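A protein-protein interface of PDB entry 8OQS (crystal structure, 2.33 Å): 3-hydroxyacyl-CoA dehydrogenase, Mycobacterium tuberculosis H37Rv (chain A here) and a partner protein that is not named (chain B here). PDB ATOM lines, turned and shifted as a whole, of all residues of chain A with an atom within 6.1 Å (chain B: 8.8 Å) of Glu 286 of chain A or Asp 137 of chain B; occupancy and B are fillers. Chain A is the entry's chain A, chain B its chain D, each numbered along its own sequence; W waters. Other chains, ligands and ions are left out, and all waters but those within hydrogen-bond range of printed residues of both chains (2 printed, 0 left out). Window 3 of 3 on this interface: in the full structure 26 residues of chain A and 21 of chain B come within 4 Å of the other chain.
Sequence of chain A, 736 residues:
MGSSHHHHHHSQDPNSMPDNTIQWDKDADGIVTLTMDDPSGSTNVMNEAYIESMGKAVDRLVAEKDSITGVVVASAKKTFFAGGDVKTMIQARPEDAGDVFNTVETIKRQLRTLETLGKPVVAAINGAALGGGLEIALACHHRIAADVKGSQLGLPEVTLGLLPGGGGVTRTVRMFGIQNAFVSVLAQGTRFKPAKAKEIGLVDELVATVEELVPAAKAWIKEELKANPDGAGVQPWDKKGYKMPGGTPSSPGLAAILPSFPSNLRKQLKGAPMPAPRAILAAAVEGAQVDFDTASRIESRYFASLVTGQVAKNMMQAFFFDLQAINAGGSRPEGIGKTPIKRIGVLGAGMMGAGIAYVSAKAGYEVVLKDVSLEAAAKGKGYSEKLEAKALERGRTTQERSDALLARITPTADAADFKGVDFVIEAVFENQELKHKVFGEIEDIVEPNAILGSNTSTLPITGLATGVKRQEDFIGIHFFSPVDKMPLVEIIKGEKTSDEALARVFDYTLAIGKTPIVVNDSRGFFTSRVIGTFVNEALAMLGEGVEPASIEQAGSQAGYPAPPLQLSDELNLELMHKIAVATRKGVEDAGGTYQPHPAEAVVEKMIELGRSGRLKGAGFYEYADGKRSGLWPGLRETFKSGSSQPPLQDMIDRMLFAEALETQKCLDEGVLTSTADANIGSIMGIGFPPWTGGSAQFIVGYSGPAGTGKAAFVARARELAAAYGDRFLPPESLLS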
ATOM      1  N   PRO A 249     -23.208 -22.430  -5.902  1.00  0.00           N
ATOM      2  CA  PRO A 249     -22.320 -21.988  -6.989  1.00  0.00           C
ATOM      3  C   PRO A 249     -23.021 -21.821  -8.326  1.00  0.00           C
ATOM      4  O   PRO A 249     -22.582 -21.005  -9.146  1.00  0.00           O
ATOM      5  CB  PRO A 249     -21.260 -23.094  -7.039  1.00  0.00           C
ATOM      6  CG  PRO A 249     -21.187 -23.577  -5.641  1.00  0.00           C
ATOM      7  CD  PRO A 249     -22.598 -23.519  -5.115  1.00  0.00           C
ATOM      8  N   LEU A 258     -18.132 -15.353  -7.366  1.00  0.00           N
ATOM      9  CA  LEU A 258     -17.367 -16.519  -6.933  1.00  0.00           C
ATOM     10  C   LEU A 258     -15.920 -16.535  -7.416  1.00  0.00           C
ATOM     11  O   LEU A 258     -15.052 -16.968  -6.639  1.00  0.00           O
ATOM     12  CB  LEU A 258     -18.094 -17.795  -7.368  1.00  0.00           C
ATOM     13  CG  LEU A 258     -17.670 -19.087  -6.674  1.00  0.00           C
ATOM     14  CD1 LEU A 258     -17.670 -18.893  -5.172  1.00  0.00           C
ATOM     15  CD2 LEU A 258     -18.611 -20.212  -7.059  1.00  0.00           C
ATOM     16  N   PRO A 262     -11.085 -16.746  -4.521  1.00  0.00           N
ATOM     17  CA  PRO A 262      -9.668 -17.124  -4.398  1.00  0.00           C
ATOM     18  C   PRO A 262      -8.720 -15.955  -4.569  1.00  0.00           C
ATOM     19  O   PRO A 262      -7.648 -15.953  -3.951  1.00  0.00           O
ATOM     20  CB  PRO A 262      -9.480 -18.164  -5.511  1.00  0.00           C
ATOM     21  CG  PRO A 262     -10.850 -18.662  -5.803  1.00  0.00           C
ATOM     22  CD  PRO A 262     -11.726 -17.464  -5.638  1.00  0.00           C
ATOM     23  N   LEU A 281     -11.642 -23.096   1.544  1.00  0.00           N
ATOM     24  CA  LEU A 281     -12.431 -22.493   0.474  1.00  0.00           C
ATOM     25  C   LEU A 281     -12.819 -23.529  -0.572  1.00  0.00           C
ATOM     26  O   LEU A 281     -13.932 -23.490  -1.112  1.00  0.00           O
ATOM     27  CB  LEU A 281     -11.648 -21.348  -0.165  1.00  0.00           C
ATOM     28  CG  LEU A 281     -12.412 -20.527  -1.198  1.00  0.00           C
ATOM     29  CD1 LEU A 281     -13.676 -19.943  -0.576  1.00  0.00           C
ATOM     30  CD2 LEU A 281     -11.523 -19.430  -1.749  1.00  0.00           C
ATOM     31  N   ALA A 282     -11.915 -24.465  -0.868  1.00  0.00           N
ATOM     32  CA  ALA A 282     -12.219 -25.514  -1.833  1.00  0.00           C
ATOM     33  C   ALA A 282     -13.289 -26.455  -1.299  1.00  0.00           C
ATOM     34  O   ALA A 282     -14.257 -26.770  -2.002  1.00  0.00           O
ATOM     35  CB  ALA A 282     -10.949 -26.287  -2.183  1.00  0.00           C
ATOM     36  N   ALA A 283     -13.129 -26.924  -0.058  1.00  0.00           N
ATOM     37  CA  ALA A 283     -14.156 -27.767   0.545  1.00  0.00           C
ATOM     38  C   ALA A 283     -15.488 -27.038   0.620  1.00  0.00           C
ATOM     39  O   ALA A 283     -16.542 -27.635   0.373  1.00  0.00           O
ATOM     40  CB  ALA A 283     -13.726 -28.218   1.940  1.00  0.00           C
ATOM     41  N   ALA A 284     -15.461 -25.746   0.951  1.00  0.00           N
ATOM     42  CA  ALA A 284     -16.705 -24.999   1.087  1.00  0.00           C
ATOM     43  C   ALA A 284     -17.452 -24.940  -0.239  1.00  0.00           C
ATOM     44  O   ALA A 284     -18.628 -25.313  -0.318  1.00  0.00           O
ATOM     45  CB  ALA A 284     -16.425 -23.594   1.620  1.00  0.00           C
ATOM     46  N   VAL A 285     -16.773 -24.503  -1.301  1.00  0.00           N
ATOM     47  CA  VAL A 285     -17.433 -24.355  -2.595  1.00  0.00           C
ATOM     48  C   VAL A 285     -17.821 -25.715  -3.163  1.00  0.00           C
ATOM     49  O   VAL A 285     -18.971 -25.926  -3.571  1.00  0.00           O
ATOM     50  CB  VAL A 285     -16.533 -23.578  -3.567  1.00  0.00           C
ATOM     51  CG1 VAL A 285     -17.176 -23.538  -4.939  1.00  0.00           C
ATOM     52  CG2 VAL A 285     -16.289 -22.174  -3.044  1.00  0.00           C
ATOM     53  N   GLU A 286     -16.867 -26.653  -3.208  1.00  0.00           N
ATOM     54  CA  GLU A 286     -17.142 -27.967  -3.785  1.00  0.00           C
ATOM     55  C   GLU A 286     -18.281 -28.662  -3.052  1.00  0.00           C
ATOM     56  O   GLU A 286     -19.107 -29.343  -3.673  1.00  0.00           O
ATOM     57  CB  GLU A 286     -15.885 -28.840  -3.753  1.00  0.00           C
ATOM     58  CG  GLU A 286     -14.742 -28.363  -4.640  1.00  0.00           C
ATOM     59  CD  GLU A 286     -13.528 -29.292  -4.598  1.00  0.00           C
ATOM     60  OE1 GLU A 286     -13.710 -30.509  -4.375  1.00  0.00           O
ATOM     61  OE2 GLU A 286     -12.393 -28.798  -4.787  1.00  0.00           O
ATOM     62  N   GLY A 287     -18.343 -28.503  -1.731  1.00  0.00           N
ATOM     63  CA  GLY A 287     -19.408 -29.131  -0.974  1.00  0.00           C
ATOM     64  C   GLY A 287     -20.770 -28.526  -1.243  1.00  0.00           C
ATOM     65  O   GLY A 287     -21.787 -29.220  -1.159  1.00  0.00           O
ATOM     66  N   ALA A 288     -20.819 -27.233  -1.573  1.00  0.00           N
ATOM     67  CA  ALA A 288     -22.102 -26.602  -1.851  1.00  0.00           C
ATOM     68  C   ALA A 288     -22.669 -27.002  -3.204  1.00  0.00           C
ATOM     69  O   ALA A 288     -23.804 -26.626  -3.517  1.00  0.00           O
ATOM     70  CB  ALA A 288     -21.976 -25.081  -1.775  1.00  0.00           C
ATOM     71  N   GLN A 289     -21.916 -27.754  -4.004  1.00  0.00           N
ATOM     72  CA  GLN A 289     -22.381 -28.212  -5.304  1.00  0.00           C
ATOM     73  C   GLN A 289     -23.073 -29.566  -5.253  1.00  0.00           C
ATOM     74  O   GLN A 289     -23.768 -29.928  -6.210  1.00  0.00           O
ATOM     75  CB  GLN A 289     -21.208 -28.301  -6.281  1.00  0.00           C
ATOM     76  CG  GLN A 289     -20.475 -26.995  -6.518  1.00  0.00           C
ATOM     77  CD  GLN A 289     -19.392 -27.132  -7.580  1.00  0.00           C
ATOM     78  OE1 GLN A 289     -18.228 -27.387  -7.269  1.00  0.00           O
ATOM     79  NE2 GLN A 289     -19.777 -26.974  -8.842  1.00  0.00           N
ATOM     80  N   VAL A 290     -22.900 -30.321  -4.170  1.00  0.00           N
ATOM     81  CA  VAL A 290     -23.364 -31.695  -4.070  1.00  0.00           C
ATOM     82  C   VAL A 290     -24.189 -31.845  -2.795  1.00  0.00           C
ATOM     83  O   VAL A 290     -24.285 -30.927  -1.984  1.00  0.00           O
ATOM     84  CB  VAL A 290     -22.197 -32.701  -4.082  1.00  0.00           C
ATOM     85  CG1 VAL A 290     -21.478 -32.673  -5.424  1.00  0.00           C
ATOM     86  CG2 VAL A 290     -21.241 -32.372  -2.959  1.00  0.00           C
ATOM     87  N   ALA A 295     -20.819 -33.902   0.125  1.00  0.00           N
ATOM     88  CA  ALA A 295     -20.058 -32.736   0.561  1.00  0.00           C
ATOM     89  C   ALA A 295     -19.209 -33.060   1.779  1.00  0.00           C
ATOM     90  O   ALA A 295     -18.054 -32.625   1.875  1.00  0.00           O
ATOM     91  CB  ALA A 295     -21.008 -31.583   0.869  1.00  0.00           C
ATOM     92  N   ILE A 298     -16.025 -35.047   0.719  1.00  0.00           N
ATOM     93  CA  ILE A 298     -15.044 -34.111   0.170  1.00  0.00           C
ATOM     94  C   ILE A 298     -14.326 -33.375   1.294  1.00  0.00           C
ATOM     95  O   ILE A 298     -13.110 -33.154   1.238  1.00  0.00           O
ATOM     96  CB  ILE A 298     -15.735 -33.124  -0.791  1.00  0.00           C
ATOM     97  CG1 ILE A 298     -16.385 -33.869  -1.959  1.00  0.00           C
ATOM     98  CG2 ILE A 298     -14.756 -32.069  -1.270  1.00  0.00           C
ATOM     99  CD1 ILE A 298     -17.244 -32.987  -2.843  1.00  0.00           C
ATOM    100  N   TYR A 302      -9.971 -33.203   2.037  1.00  0.00           N
ATOM    101  CA  TYR A 302      -9.141 -32.019   2.249  1.00  0.00           C
ATOM    102  C   TYR A 302      -8.538 -32.014   3.646  1.00  0.00           C
ATOM    103  O   TYR A 302      -7.381 -31.620   3.824  1.00  0.00           O
ATOM    104  CB  TYR A 302      -9.949 -30.745   2.007  1.00  0.00           C
ATOM    105  CG  TYR A 302     -10.077 -30.385   0.539  1.00  0.00           C
ATOM    106  CD1 TYR A 302      -9.001 -29.852  -0.159  1.00  0.00           C
ATOM    107  CD2 TYR A 302     -11.273 -30.575  -0.147  1.00  0.00           C
ATOM    108  CE1 TYR A 302      -9.105 -29.521  -1.496  1.00  0.00           C
ATOM    109  CE2 TYR A 302     -11.389 -30.244  -1.487  1.00  0.00           C
ATOM    110  CZ  TYR A 302     -10.301 -29.717  -2.157  1.00  0.00           C
ATOM    111  OH  TYR A 302     -10.403 -29.386  -3.496  1.00  0.00           O
ATOM    112  N   GLY B 131     -20.389 -20.659 -16.790  1.00  0.00           N
ATOM    113  CA  GLY B 131     -19.564 -21.088 -15.675  1.00  0.00           C
ATOM    114  C   GLY B 131     -18.167 -21.464 -16.141  1.00  0.00           C
ATOM    115  O   GLY B 131     -17.669 -20.985 -17.165  1.00  0.00           O
ATOM    116  N   GLY B 132     -17.530 -22.338 -15.383  1.00  0.00           N
ATOM    117  CA  GLY B 132     -16.200 -22.816 -15.716  1.00  0.00           C
ATOM    118  C   GLY B 132     -15.375 -23.081 -14.473  1.00  0.00           C
ATOM    119  O   GLY B 132     -15.563 -22.481 -13.419  1.00  0.00           O
ATOM    120  N   ALA B 133     -14.422 -24.004 -14.605  1.00  0.00           N
ATOM    121  CA  ALA B 133     -13.601 -24.383 -13.459  1.00  0.00           C
ATOM    122  C   ALA B 133     -12.580 -23.300 -13.122  1.00  0.00           C
ATOM    123  O   ALA B 133     -12.463 -22.886 -11.962  1.00  0.00           O
ATOM    124  CB  ALA B 133     -12.908 -25.718 -13.733  1.00  0.00           C
ATOM    125  N   MET B 134     -11.841 -22.816 -14.127  1.00  0.00           N
ATOM    126  CA  MET B 134     -10.810 -21.799 -13.918  1.00  0.00           C
ATOM    127  C   MET B 134     -11.311 -20.569 -13.171  1.00  0.00           C
ATOM    128  O   MET B 134     -10.490 -19.770 -12.707  1.00  0.00           O
ATOM    129  CB  MET B 134     -10.222 -21.351 -15.257  1.00  0.00           C
ATOM    130  CG  MET B 134      -9.282 -22.348 -15.909  1.00  0.00           C
ATOM    131  SD  MET B 134      -8.670 -21.731 -17.492  1.00  0.00           S
ATOM    132  CE  MET B 134     -10.157 -21.818 -18.489  1.00  0.00           C
ATOM    133  N   GLY B 135     -12.621 -20.385 -13.053  1.00  0.00           N
ATOM    134  CA  GLY B 135     -13.142 -19.269 -12.294  1.00  0.00           C
ATOM    135  C   GLY B 135     -13.889 -19.688 -11.050  1.00  0.00           C
ATOM    136  O   GLY B 135     -13.771 -19.043 -10.005  1.00  0.00           O
ATOM    137  N   LEU B 136     -14.657 -20.773 -11.135  1.00  0.00           N
ATOM    138  CA  LEU B 136     -15.564 -21.149 -10.053  1.00  0.00           C
ATOM    139  C   LEU B 136     -15.110 -22.366  -9.261  1.00  0.00           C
ATOM    140  O   LEU B 136     -15.869 -22.850  -8.419  1.00  0.00           O
ATOM    141  CB  LEU B 136     -16.965 -21.397 -10.621  1.00  0.00           C
ATOM    142  CG  LEU B 136     -17.514 -20.350 -11.591  1.00  0.00           C
ATOM    143  CD1 LEU B 136     -18.863 -20.800 -12.121  1.00  0.00           C
ATOM    144  CD2 LEU B 136     -17.629 -18.994 -10.927  1.00  0.00           C
ATOM    145  N   ASP B 137     -13.908 -22.884  -9.514  1.00  0.00           N
ATOM    146  CA  ASP B 137     -13.349 -23.937  -8.673  1.00  0.00           C
ATOM    147  C   ASP B 137     -12.155 -23.367  -7.923  1.00  0.00           C
ATOM    148  O   ASP B 137     -11.114 -23.102  -8.547  1.00  0.00           O
ATOM    149  CB  ASP B 137     -12.931 -25.147  -9.506  1.00  0.00           C
ATOM    150  CG  ASP B 137     -12.162 -26.167  -8.693  1.00  0.00           C
ATOM    151  OD1 ASP B 137     -12.703 -26.635  -7.669  1.00  0.00           O
ATOM    152  OD2 ASP B 137     -11.016 -26.495  -9.068  1.00  0.00           O
ATOM    153  N   PRO B 138     -12.247 -23.145  -6.611  1.00  0.00           N
ATOM    154  CA  PRO B 138     -11.191 -22.380  -5.937  1.00  0.00           C
ATOM    155  C   PRO B 138      -9.833 -23.048  -5.981  1.00  0.00           C
ATOM    156  O   PRO B 138      -8.819 -22.345  -6.024  1.00  0.00           O
ATOM    157  CB  PRO B 138     -11.724 -22.246  -4.506  1.00  0.00           C
ATOM    158  CG  PRO B 138     -13.187 -22.359  -4.654  1.00  0.00           C
ATOM    159  CD  PRO B 138     -13.388 -23.390  -5.721  1.00  0.00           C
ATOM    160  N   ALA B 139      -9.773 -24.379  -5.999  1.00  0.00           N
ATOM    161  CA  ALA B 139      -8.480 -25.051  -6.105  1.00  0.00           C
ATOM    162  C   ALA B 139      -7.802 -24.725  -7.432  1.00  0.00           C
ATOM    163  O   ALA B 139      -6.629 -24.341  -7.466  1.00  0.00           O
ATOM    164  CB  ALA B 139      -8.659 -26.559  -5.937  1.00  0.00           C
ATOM    165  N   THR B 140      -8.531 -24.864  -8.542  1.00  0.00           N
ATOM    166  CA  THR B 140      -7.983 -24.495  -9.845  1.00  0.00           C
ATOM    167  C   THR B 140      -7.677 -23.003  -9.905  1.00  0.00           C
ATOM    168  O   THR B 140      -6.572 -22.601 -10.284  1.00  0.00           O
ATOM    169  CB  THR B 140      -8.965 -24.887 -10.953  1.00  0.00           C
ATOM    170  OG1 THR B 140      -9.218 -26.296 -10.890  1.00  0.00           O
ATOM    171  CG2 THR B 140      -8.409 -24.527 -12.331  1.00  0.00           C
ATOM    172  N   ASN B 141      -8.651 -22.167  -9.530  1.00  0.00           N
ATOM    173  CA  ASN B 141      -8.482 -20.713  -9.571  1.00  0.00           C
ATOM    174  C   ASN B 141      -7.248 -20.277  -8.786  1.00  0.00           C
ATOM    175  O   ASN B 141      -6.393 -19.555  -9.310  1.00  0.00           O
ATOM    176  CB  ASN B 141      -9.751 -20.044  -9.035  1.00  0.00           C
ATOM    177  CG  ASN B 141      -9.774 -18.534  -9.220  1.00  0.00           C
ATOM    178  OD1 ASN B 141      -8.778 -17.844  -9.000  1.00  0.00           O
ATOM    179  ND2 ASN B 141     -10.930 -18.010  -9.618  1.00  0.00           N
ATOM    180  N   TYR B 142      -7.127 -20.735  -7.535  1.00  0.00           N
ATOM    181  CA  TYR B 142      -6.037 -20.303  -6.661  1.00  0.00           C
ATOM    182  C   TYR B 142      -4.669 -20.656  -7.222  1.00  0.00           C
ATOM    183  O   TYR B 142      -3.675 -20.005  -6.884  1.00  0.00           O
ATOM    184  CB  TYR B 142      -6.208 -20.944  -5.284  1.00  0.00           C
ATOM    185  CG  TYR B 142      -5.431 -20.312  -4.152  1.00  0.00           C
ATOM    186  CD1 TYR B 142      -4.104 -20.663  -3.901  1.00  0.00           C
ATOM    187  CD2 TYR B 142      -6.043 -19.397  -3.300  1.00  0.00           C
ATOM    188  CE1 TYR B 142      -3.402 -20.094  -2.843  1.00  0.00           C
ATOM    189  CE2 TYR B 142      -5.354 -18.829  -2.244  1.00  0.00           C
ATOM    190  CZ  TYR B 142      -4.038 -19.179  -2.020  1.00  0.00           C
ATOM    191  OH  TYR B 142      -3.367 -18.604  -0.967  1.00  0.00           O
ATOM    192  N   ASP B 143      -4.591 -21.681  -8.067  1.00  0.00           N
ATOM    193  CA  ASP B 143      -3.314 -22.191  -8.550  1.00  0.00           C
ATOM    194  C   ASP B 143      -2.922 -21.643  -9.913  1.00  0.00           C
ATOM    195  O   ASP B 143      -1.762 -21.274 -10.109  1.00  0.00           O
ATOM    196  CB  ASP B 143      -3.348 -23.721  -8.600  1.00  0.00           C
ATOM    197  CG  ASP B 143      -3.506 -24.338  -7.224  1.00  0.00           C
ATOM    198  OD1 ASP B 143      -3.473 -23.581  -6.225  1.00  0.00           O
ATOM    199  OD2 ASP B 143      -3.666 -25.575  -7.142  1.00  0.00           O
ATOM    200  N   VAL B 144      -3.860 -21.579 -10.864  1.00  0.00           N
ATOM    201  CA  VAL B 144      -3.553 -21.005 -12.175  1.00  0.00           C
ATOM    202  C   VAL B 144      -3.462 -19.489 -12.147  1.00  0.00           C
ATOM    203  O   VAL B 144      -3.114 -18.883 -13.171  1.00  0.00           O
ATOM    204  CB  VAL B 144      -4.601 -21.408 -13.230  1.00  0.00           C
ATOM    205  CG1 VAL B 144      -4.857 -22.904 -13.177  1.00  0.00           C
ATOM    206  CG2 VAL B 144      -5.893 -20.616 -13.038  1.00  0.00           C
ATOM    207  N   PHE B 146      -5.946 -17.006 -11.681  1.00  0.00           N
ATOM    208  CA  PHE B 146      -6.964 -16.472 -12.575  1.00  0.00           C
ATOM    209  C   PHE B 146      -7.044 -14.955 -12.464  1.00  0.00           C
ATOM    210  O   PHE B 146      -7.081 -14.399 -11.362  1.00  0.00           O
ATOM    211  CB  PHE B 146      -8.325 -17.095 -12.262  1.00  0.00           C
ATOM    212  CG  PHE B 146      -9.464 -16.474 -13.025  1.00  0.00           C
ATOM    213  CD1 PHE B 146      -9.748 -16.880 -14.319  1.00  0.00           C
ATOM    214  CD2 PHE B 146     -10.250 -15.486 -12.449  1.00  0.00           C
ATOM    215  CE1 PHE B 146     -10.786 -16.313 -15.025  1.00  0.00           C
ATOM    216  CE2 PHE B 146     -11.292 -14.914 -13.150  1.00  0.00           C
ATOM    217  CZ  PHE B 146     -11.560 -15.329 -14.440  1.00  0.00           C
HETATM  218  O   HOH W   1     -11.546 -29.892  -7.697  1.00  0.00           O
HETATM  219  O   HOH W   2     -12.108 -26.392  -5.216  1.00  0.00           O
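Water W2 lies within hydrogen-bond range of the side-chain carboxylate (OE2) of Glu 286 of chain A (2.5 Å), the side-chain carboxylate (OD1) of Asp 137 of chain B (2.5 Å) and the backbone NH (N) of Ala 139 of chain B (3.2 Å). Water W1 lies within hydrogen-bond range of the side-chain carboxylate (OE2) of Glu 286 of chain A and the side-chain carboxylate (OD1) of Asp 137 of chain B.
Leu 136 of chain B touches Leu 258 of chain A. Pro 138 of chain B touches Pro 262 of chain A. CB of Pro 262 of chain A touches OD1 of Asn 141 of chain B (3.6 Å). CD2 of Tyr 142 of chain B touches O of Pro 262 of chain A, 3.9 Å away. Pro 138 of chain B touches Leu 281 of chain A. Leu 136 of chain B touches Val 285 of chain A. Pro 138 of chain B touches Val 285 of chain A (CG to CG2, 3.5 Å). OE2 of Glu 286 of chain A touches OD1 of Asp 137 of chain B, at 3.6 Å.
Of the 16 printed residues of chain A, 5 touch a printed residue of chain B. Along chain A the printed residues that touch a printed residue of chain B span positions 258 to 286. Of the 15 printed residues of chain B, 5 touch a printed residue of chain A. Printed residues of chain B that touch a printed residue of chain A: Leu 136, Asp 137, Pro 138, Asn 141 and Tyr 142. Hydrophobic or aromatic side chains of chain B within 4 Å of the printed part of chain A: Leu 136, Pro 138 and Tyr 142. Among the printed residues, 8 pairs touch across the chains.
The backbone carbonyl oxygen of Gly 135 of chain B is in hydrogen-bond range of the side-chain amide nitrogen of Asn 141 of chain B (3.0 Å). OD2 of Asp 137 of chain B sits at hydrogen-bond distance from OG1 of Thr 140 of chain B (2.6 Å). OE2 of Glu 286 of chain A is in hydrogen-bond range of OH of Tyr 302 of chain A (2.4 Å).
Of the printed residues of chain B, Leu 258 of chain A touches Leu 136. Of the printed residues of chain B, Pro 262 of chain A touches Pro 138, Asn 141 and Tyr 142. Of the printed residues of chain B, Leu 281 of chain A touches Pro 138 (3.8 Å). Glu 286 of chain A touches one residue of chain B. Gly 287 of chain A touches none of the printed residues of chain B. Printed residues of chain A within 4 Å of Leu 136 of chain B: Leu 258 and Val 285. Printed residues of chain A within 4 Å of Asp 137 of chain B: Glu 286 (3.6 Å). Printed residues of chain A within 4 Å of Pro 138 of chain B: Pro 262 (3.7 Å), Leu 281 (3.8 Å) and Val 285 (3.5 Å). The nearest printed residue of chain A that does not touch Tyr 142 of chain B is Leu 281 of chain A (5.7 Å).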
